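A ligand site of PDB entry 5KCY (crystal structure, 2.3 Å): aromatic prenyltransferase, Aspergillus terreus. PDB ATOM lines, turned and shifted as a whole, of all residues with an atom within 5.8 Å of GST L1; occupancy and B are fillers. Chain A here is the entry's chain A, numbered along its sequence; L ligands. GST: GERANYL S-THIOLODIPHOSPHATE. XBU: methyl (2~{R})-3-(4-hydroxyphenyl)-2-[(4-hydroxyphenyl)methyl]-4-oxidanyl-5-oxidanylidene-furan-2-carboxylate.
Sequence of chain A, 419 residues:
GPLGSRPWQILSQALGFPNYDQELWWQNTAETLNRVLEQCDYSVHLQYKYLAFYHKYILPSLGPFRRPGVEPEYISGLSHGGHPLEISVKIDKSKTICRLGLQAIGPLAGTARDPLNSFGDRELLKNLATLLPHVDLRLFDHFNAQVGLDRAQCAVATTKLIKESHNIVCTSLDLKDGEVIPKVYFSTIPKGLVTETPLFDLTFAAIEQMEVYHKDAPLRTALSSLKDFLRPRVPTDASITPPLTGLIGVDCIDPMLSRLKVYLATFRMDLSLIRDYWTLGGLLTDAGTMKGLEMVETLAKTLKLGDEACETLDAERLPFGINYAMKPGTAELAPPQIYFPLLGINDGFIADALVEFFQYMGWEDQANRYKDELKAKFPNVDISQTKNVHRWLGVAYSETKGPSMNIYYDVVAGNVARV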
ATOM      1  N   SER A  88      17.469 -11.873 -11.063  1.00  0.00           N
ATOM      2  CA  SER A  88      16.057 -11.883 -11.342  1.00  0.00           C
ATOM      3  C   SER A  88      15.518 -13.297 -11.336  1.00  0.00           C
ATOM      4  O   SER A  88      16.262 -14.258 -11.541  1.00  0.00           O
ATOM      5  CB  SER A  88      15.764 -11.128 -12.646  1.00  0.00           C
ATOM      6  OG  SER A  88      16.304 -11.779 -13.766  1.00  0.00           O
ATOM      7  N   LYS A  90      12.338 -15.640 -13.017  1.00  0.00           N
ATOM      8  CA  LYS A  90      11.221 -15.775 -13.950  1.00  0.00           C
ATOM      9  C   LYS A  90      10.329 -16.910 -13.372  1.00  0.00           C
ATOM     10  O   LYS A  90      10.738 -18.068 -13.314  1.00  0.00           O
ATOM     11  CB  LYS A  90      11.702 -16.104 -15.347  1.00  0.00           C
ATOM     12  CG  LYS A  90      10.578 -16.203 -16.391  1.00  0.00           C
ATOM     13  CD  LYS A  90      11.132 -16.580 -17.765  1.00  0.00           C
ATOM     14  CE  LYS A  90      10.327 -15.943 -18.910  1.00  0.00           C
ATOM     15  NZ  LYS A  90      10.658 -14.492 -19.167  1.00  0.00           N
ATOM     16  N   ARG A  99      18.236 -15.606 -13.307  1.00  0.00           N
ATOM     17  CA  ARG A  99      19.004 -14.891 -14.300  1.00  0.00           C
ATOM     18  C   ARG A  99      19.881 -13.805 -13.628  1.00  0.00           C
ATOM     19  O   ARG A  99      19.476 -13.202 -12.637  1.00  0.00           O
ATOM     20  CB  ARG A  99      18.032 -14.329 -15.316  1.00  0.00           C
ATOM     21  CG  ARG A  99      18.706 -13.392 -16.265  1.00  0.00           C
ATOM     22  CD  ARG A  99      17.855 -12.712 -17.341  1.00  0.00           C
ATOM     23  NE  ARG A  99      17.092 -13.712 -18.089  1.00  0.00           N
ATOM     24  CZ  ARG A  99      16.540 -13.484 -19.284  1.00  0.00           C
ATOM     25  NH1 ARG A  99      16.692 -12.318 -19.911  1.00  0.00           N
ATOM     26  NH2 ARG A  99      15.866 -14.461 -19.866  1.00  0.00           N
ATOM     27  N   SER A 172      23.241  -9.969 -19.692  1.00  0.00           N
ATOM     28  CA  SER A 172      22.513 -10.882 -18.799  1.00  0.00           C
ATOM     29  C   SER A 172      22.855 -12.318 -19.110  1.00  0.00           C
ATOM     30  O   SER A 172      23.098 -12.696 -20.251  1.00  0.00           O
ATOM     31  CB  SER A 172      20.981 -10.760 -19.018  1.00  0.00           C
ATOM     32  OG  SER A 172      20.503  -9.749 -18.157  1.00  0.00           O
ATOM     33  N   LYS A 183      22.815 -12.708 -23.042  1.00  0.00           N
ATOM     34  CA  LYS A 183      22.051 -11.747 -23.762  1.00  0.00           C
ATOM     35  C   LYS A 183      22.803 -10.435 -23.665  1.00  0.00           C
ATOM     36  O   LYS A 183      23.407 -10.218 -22.637  1.00  0.00           O
ATOM     37  CB  LYS A 183      20.784 -11.568 -22.974  1.00  0.00           C
ATOM     38  CG  LYS A 183      19.514 -11.699 -23.753  1.00  0.00           C
ATOM     39  CD  LYS A 183      18.830 -10.330 -23.707  1.00  0.00           C
ATOM     40  CE  LYS A 183      18.032  -9.996 -24.949  1.00  0.00           C
ATOM     41  NZ  LYS A 183      17.242  -8.766 -24.616  1.00  0.00           N
ATOM     42  N   TYR A 185      22.467  -5.913 -24.220  1.00  0.00           N
ATOM     43  CA  TYR A 185      21.584  -4.756 -24.379  1.00  0.00           C
ATOM     44  C   TYR A 185      22.444  -3.579 -24.762  1.00  0.00           C
ATOM     45  O   TYR A 185      23.477  -3.308 -24.117  1.00  0.00           O
ATOM     46  CB  TYR A 185      20.844  -4.480 -23.054  1.00  0.00           C
ATOM     47  CG  TYR A 185      20.233  -5.732 -22.437  1.00  0.00           C
ATOM     48  CD1 TYR A 185      21.007  -6.562 -21.641  1.00  0.00           C
ATOM     49  CD2 TYR A 185      18.903  -6.059 -22.625  1.00  0.00           C
ATOM     50  CE1 TYR A 185      20.483  -7.720 -21.080  1.00  0.00           C
ATOM     51  CE2 TYR A 185      18.344  -7.194 -22.063  1.00  0.00           C
ATOM     52  CZ  TYR A 185      19.145  -8.033 -21.286  1.00  0.00           C
ATOM     53  OH  TYR A 185      18.620  -9.195 -20.734  1.00  0.00           O
ATOM     54  N   LEU A 247      16.850   1.025 -25.877  1.00  0.00           N
ATOM     55  CA  LEU A 247      17.640  -0.199 -25.757  1.00  0.00           C
ATOM     56  C   LEU A 247      17.274  -1.156 -26.834  1.00  0.00           C
ATOM     57  O   LEU A 247      16.088  -1.400 -27.075  1.00  0.00           O
ATOM     58  CB  LEU A 247      17.342  -0.929 -24.482  1.00  0.00           C
ATOM     59  CG  LEU A 247      18.155  -0.944 -23.235  1.00  0.00           C
ATOM     60  CD1 LEU A 247      17.669  -2.129 -22.420  1.00  0.00           C
ATOM     61  CD2 LEU A 247      19.668  -0.956 -23.418  1.00  0.00           C
ATOM     62  N   ARG A 259      16.236 -13.837 -30.571  1.00  0.00           N
ATOM     63  CA  ARG A 259      15.180 -12.850 -30.377  1.00  0.00           C
ATOM     64  C   ARG A 259      15.817 -11.456 -30.400  1.00  0.00           C
ATOM     65  O   ARG A 259      16.847 -11.209 -29.799  1.00  0.00           O
ATOM     66  CB  ARG A 259      14.414 -13.078 -29.070  1.00  0.00           C
ATOM     67  CG  ARG A 259      13.750 -14.449 -28.899  1.00  0.00           C
ATOM     68  CD  ARG A 259      13.012 -14.576 -27.558  1.00  0.00           C
ATOM     69  NE  ARG A 259      13.844 -14.282 -26.367  1.00  0.00           N
ATOM     70  CZ  ARG A 259      13.388 -14.200 -25.098  1.00  0.00           C
ATOM     71  NH1 ARG A 259      12.099 -14.429 -24.816  1.00  0.00           N
ATOM     72  NH2 ARG A 259      14.216 -13.903 -24.091  1.00  0.00           N
ATOM     73  N   LYS A 261      14.979  -7.565 -29.508  1.00  0.00           N
ATOM     74  CA  LYS A 261      14.096  -6.827 -28.636  1.00  0.00           C
ATOM     75  C   LYS A 261      14.300  -5.329 -28.752  1.00  0.00           C
ATOM     76  O   LYS A 261      15.422  -4.847 -28.673  1.00  0.00           O
ATOM     77  CB  LYS A 261      14.313  -7.300 -27.209  1.00  0.00           C
ATOM     78  CG  LYS A 261      13.672  -8.657 -27.001  1.00  0.00           C
ATOM     79  CD  LYS A 261      13.790  -9.132 -25.568  1.00  0.00           C
ATOM     80  CE  LYS A 261      14.721 -10.314 -25.443  1.00  0.00           C
ATOM     81  NZ  LYS A 261      14.971 -10.665 -24.016  1.00  0.00           N
ATOM     82  N   TYR A 263      13.175  -1.940 -26.688  1.00  0.00           N
ATOM     83  CA  TYR A 263      12.656  -1.517 -25.410  1.00  0.00           C
ATOM     84  C   TYR A 263      12.261  -0.021 -25.484  1.00  0.00           C
ATOM     85  O   TYR A 263      13.052   0.820 -25.941  1.00  0.00           O
ATOM     86  CB  TYR A 263      13.731  -1.661 -24.333  1.00  0.00           C
ATOM     87  CG  TYR A 263      14.087  -3.071 -23.951  1.00  0.00           C
ATOM     88  CD1 TYR A 263      15.041  -3.805 -24.691  1.00  0.00           C
ATOM     89  CD2 TYR A 263      13.492  -3.691 -22.860  1.00  0.00           C
ATOM     90  CE1 TYR A 263      15.401  -5.108 -24.334  1.00  0.00           C
ATOM     91  CE2 TYR A 263      13.831  -5.005 -22.507  1.00  0.00           C
ATOM     92  CZ  TYR A 263      14.785  -5.700 -23.234  1.00  0.00           C
ATOM     93  OH  TYR A 263      15.136  -6.985 -22.887  1.00  0.00           O
ATOM     94  N   LEU A 264      11.063   0.291 -25.035  1.00  0.00           N
ATOM     95  CA  LEU A 264      10.687   1.664 -24.836  1.00  0.00           C
ATOM     96  C   LEU A 264      10.874   2.024 -23.387  1.00  0.00           C
ATOM     97  O   LEU A 264      10.559   1.232 -22.534  1.00  0.00           O
ATOM     98  CB  LEU A 264       9.216   1.881 -25.180  1.00  0.00           C
ATOM     99  CG  LEU A 264       8.730   1.682 -26.600  1.00  0.00           C
ATOM    100  CD1 LEU A 264       7.234   2.038 -26.733  1.00  0.00           C
ATOM    101  CD2 LEU A 264       9.547   2.505 -27.563  1.00  0.00           C
ATOM    102  N   ALA A 265      11.362   3.227 -23.125  1.00  0.00           N
ATOM    103  CA  ALA A 265      11.354   3.795 -21.781  1.00  0.00           C
ATOM    104  C   ALA A 265      10.420   4.974 -21.733  1.00  0.00           C
ATOM    105  O   ALA A 265      10.442   5.812 -22.607  1.00  0.00           O
ATOM    106  CB  ALA A 265      12.760   4.225 -21.368  1.00  0.00           C
ATOM    107  N   THR A 266       9.595   5.033 -20.707  1.00  0.00           N
ATOM    108  CA  THR A 266       8.625   6.127 -20.575  1.00  0.00           C
ATOM    109  C   THR A 266       8.290   6.359 -19.133  1.00  0.00           C
ATOM    110  O   THR A 266       8.421   5.444 -18.326  1.00  0.00           O
ATOM    111  CB  THR A 266       7.353   5.863 -21.418  1.00  0.00           C
ATOM    112  OG1 THR A 266       6.578   7.070 -21.542  1.00  0.00           O
ATOM    113  CG2 THR A 266       6.470   4.697 -20.823  1.00  0.00           C
ATOM    114  N   PRO A 319      12.008   4.860 -15.235  1.00  0.00           N
ATOM    115  CA  PRO A 319      10.919   4.787 -16.146  1.00  0.00           C
ATOM    116  C   PRO A 319      10.223   3.432 -16.164  1.00  0.00           C
ATOM    117  O   PRO A 319      10.745   2.449 -15.695  1.00  0.00           O
ATOM    118  CB  PRO A 319      11.596   5.100 -17.495  1.00  0.00           C
ATOM    119  CG  PRO A 319      13.037   4.809 -17.326  1.00  0.00           C
ATOM    120  CD  PRO A 319      13.318   5.010 -15.897  1.00  0.00           C
ATOM    121  N   PHE A 320       9.039   3.375 -16.771  1.00  0.00           N
ATOM    122  CA  PHE A 320       8.398   2.122 -17.123  1.00  0.00           C
ATOM    123  C   PHE A 320       9.119   1.621 -18.357  1.00  0.00           C
ATOM    124  O   PHE A 320       9.551   2.442 -19.140  1.00  0.00           O
ATOM    125  CB  PHE A 320       6.895   2.310 -17.415  1.00  0.00           C
ATOM    126  CG  PHE A 320       6.083   2.691 -16.201  1.00  0.00           C
ATOM    127  CD1 PHE A 320       5.975   4.014 -15.793  1.00  0.00           C
ATOM    128  CD2 PHE A 320       5.394   1.735 -15.491  1.00  0.00           C
ATOM    129  CE1 PHE A 320       5.237   4.364 -14.658  1.00  0.00           C
ATOM    130  CE2 PHE A 320       4.640   2.087 -14.379  1.00  0.00           C
ATOM    131  CZ  PHE A 320       4.577   3.396 -13.943  1.00  0.00           C
ATOM    132  N   GLY A 321       9.190   0.312 -18.542  1.00  0.00           N
ATOM    133  CA  GLY A 321       9.752  -0.287 -19.749  1.00  0.00           C
ATOM    134  C   GLY A 321       8.709  -1.086 -20.502  1.00  0.00           C
ATOM    135  O   GLY A 321       7.853  -1.731 -19.887  1.00  0.00           O
ATOM    136  N   ILE A 322       8.747  -0.999 -21.832  1.00  0.00           N
ATOM    137  CA  ILE A 322       7.941  -1.849 -22.672  1.00  0.00           C
ATOM    138  C   ILE A 322       8.871  -2.530 -23.680  1.00  0.00           C
ATOM    139  O   ILE A 322       9.601  -1.844 -24.369  1.00  0.00           O
ATOM    140  CB  ILE A 322       6.811  -1.072 -23.398  1.00  0.00           C
ATOM    141  CG1 ILE A 322       5.997  -0.230 -22.416  1.00  0.00           C
ATOM    142  CG2 ILE A 322       5.866  -2.039 -24.098  1.00  0.00           C
ATOM    143  CD1 ILE A 322       6.500   1.187 -22.296  1.00  0.00           C
ATOM    144  N   ASN A 323       8.807  -3.858 -23.768  1.00  0.00           N
ATOM    145  CA  ASN A 323       9.813  -4.674 -24.500  1.00  0.00           C
ATOM    146  C   ASN A 323       9.072  -5.399 -25.618  1.00  0.00           C
ATOM    147  O   ASN A 323       8.278  -6.308 -25.329  1.00  0.00           O
ATOM    148  CB  ASN A 323      10.405  -5.660 -23.472  1.00  0.00           C
ATOM    149  CG  ASN A 323      11.340  -6.726 -24.063  1.00  0.00           C
ATOM    150  OD1 ASN A 323      11.665  -6.766 -25.257  1.00  0.00           O
ATOM    151  ND2 ASN A 323      11.808  -7.588 -23.177  1.00  0.00           N
ATOM    152  N   GLN A 337       6.260  -7.170 -23.142  1.00  0.00           N
ATOM    153  CA  GLN A 337       6.359  -7.333 -21.697  1.00  0.00           C
ATOM    154  C   GLN A 337       6.455  -5.928 -21.162  1.00  0.00           C
ATOM    155  O   GLN A 337       7.130  -5.064 -21.786  1.00  0.00           O
ATOM    156  CB  GLN A 337       7.596  -8.157 -21.304  1.00  0.00           C
ATOM    157  CG  GLN A 337       7.492  -9.583 -21.862  1.00  0.00           C
ATOM    158  CD  GLN A 337       8.709 -10.463 -21.598  1.00  0.00           C
ATOM    159  OE1 GLN A 337       9.156 -11.173 -22.509  1.00  0.00           O
ATOM    160  NE2 GLN A 337       9.236 -10.427 -20.375  1.00  0.00           N
ATOM    161  N   TYR A 339       7.457  -3.515 -17.890  1.00  0.00           N
ATOM    162  CA  TYR A 339       8.282  -3.498 -16.672  1.00  0.00           C
ATOM    163  C   TYR A 339       7.857  -2.305 -15.811  1.00  0.00           C
ATOM    164  O   TYR A 339       7.958  -1.159 -16.219  1.00  0.00           O
ATOM    165  CB  TYR A 339       9.789  -3.459 -17.043  1.00  0.00           C
ATOM    166  CG  TYR A 339      10.214  -4.721 -17.809  1.00  0.00           C
ATOM    167  CD1 TYR A 339      10.014  -4.810 -19.144  1.00  0.00           C
ATOM    168  CD2 TYR A 339      10.771  -5.821 -17.161  1.00  0.00           C
ATOM    169  CE1 TYR A 339      10.383  -5.940 -19.842  1.00  0.00           C
ATOM    170  CE2 TYR A 339      11.141  -6.964 -17.853  1.00  0.00           C
ATOM    171  CZ  TYR A 339      10.932  -7.005 -19.203  1.00  0.00           C
ATOM    172  OH  TYR A 339      11.220  -8.096 -19.953  1.00  0.00           O
ATOM    173  N   TRP A 392      12.438  -4.100 -10.387  1.00  0.00           N
ATOM    174  CA  TRP A 392      11.547  -4.150 -11.538  1.00  0.00           C
ATOM    175  C   TRP A 392      10.683  -5.317 -11.332  1.00  0.00           C
ATOM    176  O   TRP A 392      11.068  -6.303 -10.693  1.00  0.00           O
ATOM    177  CB  TRP A 392      12.258  -4.396 -12.867  1.00  0.00           C
ATOM    178  CG  TRP A 392      13.291  -3.374 -13.253  1.00  0.00           C
ATOM    179  CD1 TRP A 392      14.626  -3.482 -13.123  1.00  0.00           C
ATOM    180  CD2 TRP A 392      13.052  -2.116 -13.865  1.00  0.00           C
ATOM    181  NE1 TRP A 392      15.256  -2.368 -13.596  1.00  0.00           N
ATOM    182  CE2 TRP A 392      14.311  -1.493 -14.043  1.00  0.00           C
ATOM    183  CE3 TRP A 392      11.909  -1.436 -14.252  1.00  0.00           C
ATOM    184  CZ2 TRP A 392      14.451  -0.232 -14.585  1.00  0.00           C
ATOM    185  CZ3 TRP A 392      12.040  -0.211 -14.842  1.00  0.00           C
ATOM    186  CH2 TRP A 392      13.302   0.393 -14.997  1.00  0.00           C
ATOM    187  N   ASN A 406       8.434 -11.729 -13.721  1.00  0.00           N
ATOM    188  CA  ASN A 406       9.855 -11.477 -13.679  1.00  0.00           C
ATOM    189  C   ASN A 406      10.134 -10.467 -12.615  1.00  0.00           C
ATOM    190  O   ASN A 406       9.708  -9.338 -12.724  1.00  0.00           O
ATOM    191  CB  ASN A 406      10.301 -10.946 -15.022  1.00  0.00           C
ATOM    192  CG  ASN A 406      10.135 -11.964 -16.111  1.00  0.00           C
ATOM    193  OD1 ASN A 406      10.986 -12.818 -16.265  1.00  0.00           O
ATOM    194  ND2 ASN A 406       9.005 -11.901 -16.843  1.00  0.00           N
ATOM    195  N   TYR A 408      13.111  -8.484 -10.554  1.00  0.00           N
ATOM    196  CA  TYR A 408      14.470  -8.087 -10.566  1.00  0.00           C
ATOM    197  C   TYR A 408      14.854  -7.501  -9.182  1.00  0.00           C
ATOM    198  O   TYR A 408      14.272  -6.499  -8.756  1.00  0.00           O
ATOM    199  CB  TYR A 408      14.722  -7.063 -11.668  1.00  0.00           C
ATOM    200  CG  TYR A 408      14.536  -7.635 -13.047  1.00  0.00           C
ATOM    201  CD1 TYR A 408      13.267  -7.924 -13.510  1.00  0.00           C
ATOM    202  CD2 TYR A 408      15.632  -7.967 -13.890  1.00  0.00           C
ATOM    203  CE1 TYR A 408      13.048  -8.509 -14.731  1.00  0.00           C
ATOM    204  CE2 TYR A 408      15.433  -8.547 -15.149  1.00  0.00           C
ATOM    205  CZ  TYR A 408      14.123  -8.808 -15.557  1.00  0.00           C
ATOM    206  OH  TYR A 408      13.805  -9.370 -16.786  1.00  0.00           O
HETATM  207  PA  GST L   1      13.363 -11.297 -21.302  1.00  0.00           P
HETATM  208  O1A GST L   1      12.040 -11.911 -20.646  1.00  0.00           O
HETATM  209  O2A GST L   1      12.985 -10.132 -22.234  1.00  0.00           O
HETATM  210  O3A GST L   1      14.062 -12.411 -22.048  1.00  0.00           O
HETATM  211  O1B GST L   1      13.953 -10.544 -20.089  1.00  0.00           O
HETATM  212  PB  GST L   1      15.138  -9.445 -20.057  1.00  0.00           P
HETATM  213  O2B GST L   1      16.151  -9.530 -21.135  1.00  0.00           O
HETATM  214  O3B GST L   1      15.840  -9.807 -18.532  1.00  0.00           O
HETATM  215  S1  GST L   1      14.274  -7.501 -19.873  1.00  0.00           S
HETATM  216  C1  GST L   1      15.486  -7.048 -18.561  1.00  0.00           C
HETATM  217  C2  GST L   1      14.779  -5.905 -17.806  1.00  0.00           C
HETATM  218  C3  GST L   1      15.018  -4.503 -18.202  1.00  0.00           C
HETATM  219  C10 GST L   1      15.954  -4.274 -19.392  1.00  0.00           C
HETATM  220  C4  GST L   1      14.278  -3.357 -17.528  1.00  0.00           C
HETATM  221  C5  GST L   1      13.535  -2.727 -18.707  1.00  0.00           C
HETATM  222  C6  GST L   1      13.264  -1.271 -18.365  1.00  0.00           C
HETATM  223  C7  GST L   1      13.270  -0.180 -19.423  1.00  0.00           C
HETATM  224  C9  GST L   1      13.742  -0.453 -20.851  1.00  0.00           C
HETATM  225  C8  GST L   1      12.913   1.239 -19.010  1.00  0.00           C
HETATM  226  CAI XBU L   2      16.854   0.961 -20.356  1.00  0.00           C
HETATM  227  CAJ XBU L   2      16.787   2.063 -21.212  1.00  0.00           C
HETATM  228  CAK XBU L   2      16.566   3.328 -20.709  1.00  0.00           C
HETATM  229  OAN XBU L   2      16.498   4.319 -21.618  1.00  0.00           O
HETATM  230  CAL XBU L   2      16.420   3.482 -19.324  1.00  0.00           C
HETATM  231  CAM XBU L   2      16.510   2.367 -18.451  1.00  0.00           C
HETATM  232  CAH XBU L   2      16.760   1.068 -18.959  1.00  0.00           C
HETATM  233  CAF XBU L   2      16.878  -0.147 -18.227  1.00  0.00           C
HETATM  234  CAB XBU L   2      18.183  -0.274 -17.319  1.00  0.00           C
HETATM  235  CAX XBU L   2      19.480  -0.092 -17.953  1.00  0.00           C
HETATM  236  OAY XBU L   2      20.466   0.196 -17.258  1.00  0.00           O
HETATM  237  OAZ XBU L   2      19.562  -0.219 -19.327  1.00  0.00           O
HETATM  238  CBB XBU L   2      20.790   0.329 -19.919  1.00  0.00           C
HETATM  239  OAC XBU L   2      18.056   0.826 -16.376  1.00  0.00           O
HETATM  240  CAD XBU L   2      18.063   0.280 -15.150  1.00  0.00           C
HETATM  241  OAP XBU L   2      17.985   0.952 -14.122  1.00  0.00           O
HETATM  242  CAE XBU L   2      18.160  -1.060 -15.159  1.00  0.00           C
HETATM  243  OAO XBU L   2      18.120  -1.717 -13.938  1.00  0.00           O
HETATM  244  CAA XBU L   2      18.182  -1.505 -16.458  1.00  0.00           C
HETATM  245  CAQ XBU L   2      18.363  -2.855 -16.832  1.00  0.00           C
HETATM  246  CAR XBU L   2      18.212  -3.945 -15.949  1.00  0.00           C
HETATM  247  CAS XBU L   2      18.479  -5.279 -16.302  1.00  0.00           C
HETATM  248  CAT XBU L   2      18.917  -5.591 -17.592  1.00  0.00           C
HETATM  249  OAW XBU L   2      19.166  -6.846 -17.975  1.00  0.00           O
HETATM  250  CAU XBU L   2      19.088  -4.561 -18.511  1.00  0.00           C
HETATM  251  CAV XBU L   2      18.824  -3.237 -18.119  1.00  0.00           C
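The side-chain amide nitrogen (NE2) of Gln 337 sits at hydrogen-bond distance from an oxygen (O1A) of GST L1, at 3.2 Å. OH of Tyr 339 lies close to S1 of GST L1, at 3.1 Å. The side-chain hydroxyl of Tyr 185 is in hydrogen-bond range of an oxygen (O2B) of GST L1 (2.5 Å). OH of Tyr 408 lies within hydrogen-bond range of O3B of GST L1. NH2 of Arg 259 lies within salt-bridge range of O3A of GST L1, 2.5 Å away. The indole nitrogen (NE1) of Trp 392 sits at hydrogen-bond distance from an oxygen (OAO) of XBU L2, at 3.0 Å. An oxygen (OAW) of XBU L2 is in hydrogen-bond range of the side-chain hydroxyl (OG) of Ser 172 (3.2 Å). The side-chain amino group (NZ) of Lys 183 is in salt-bridge range of an oxygen (O2B) of GST L1, 3.7 Å away. An oxygen (O2A) of GST L1 is in salt-bridge range of the side-chain amino group (NZ) of Lys 261, at 2.7 Å. An oxygen (O1A) of GST L1 is in salt-bridge range of the side-chain amino group of Lys 90 (3.3 Å). ND2 of Asn 323 lies within hydrogen-bond range of O2A of GST L1, 3.0 Å away. O3B of GST L1 lies within salt-bridge range of NH1 of Arg 99 (3.0 Å). A sulfur (S1) of GST L1 sits close to the side-chain hydroxyl of Tyr 263 (3.2 Å).
The backbone carbonyl oxygen (O) of Ile 322 lies within hydrogen-bond range of the backbone NH (N) of Leu 264, 2.7 Å away. N of Tyr 408 is in hydrogen-bond range of O of Trp 392 (3.0 Å). The backbone carbonyl oxygen (O) of Arg 99 is in hydrogen-bond range of the backbone NH (N) of Ser 88 (2.9 Å). ND2 of Asn 323 is in hydrogen-bond range of OH of Tyr 339, 3.3 Å away. The backbone NH (N) of Tyr 339 is in hydrogen-bond range of the backbone carbonyl oxygen (O) of Gly 321 (2.7 Å). OH of Tyr 263 lies close to ND2 of Asn 323 (3.4 Å). The side-chain amino group (NZ) of Lys 90 lies within hydrogen-bond range of the side-chain amide oxygen (OD1) of Asn 406, 3.4 Å away. The backbone NH (N) of Lys 183 lies within hydrogen-bond range of the backbone carbonyl oxygen (O) of Ser 172 (2.8 Å).
Leu 264 touches GST L1. Ala 265 touches GST L1. Pro 319 touches GST L1 (CG to C8, 3.9 Å). Phe 320 touches GST L1. Gly 321 touches GST L1 (CA to C7, 3.5 Å). CH2 of Trp 392 touches C6 of GST L1 (3.8 Å). Hydrophobic or aromatic side chains within 4 Å of GST L1: Tyr 185, Tyr 263, Ala 265, Pro 319, Tyr 339, Trp 392 and Tyr 408. Within 4 Å of GST L1: Lys 90, Arg 99, Lys 183, Tyr 185, Arg 259, Lys 261, Tyr 263, Leu 264, Ala 265, Pro 319, Phe 320, Gly 321, Asn 323, Gln 337, Tyr 339, Trp 392 and Tyr 408.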
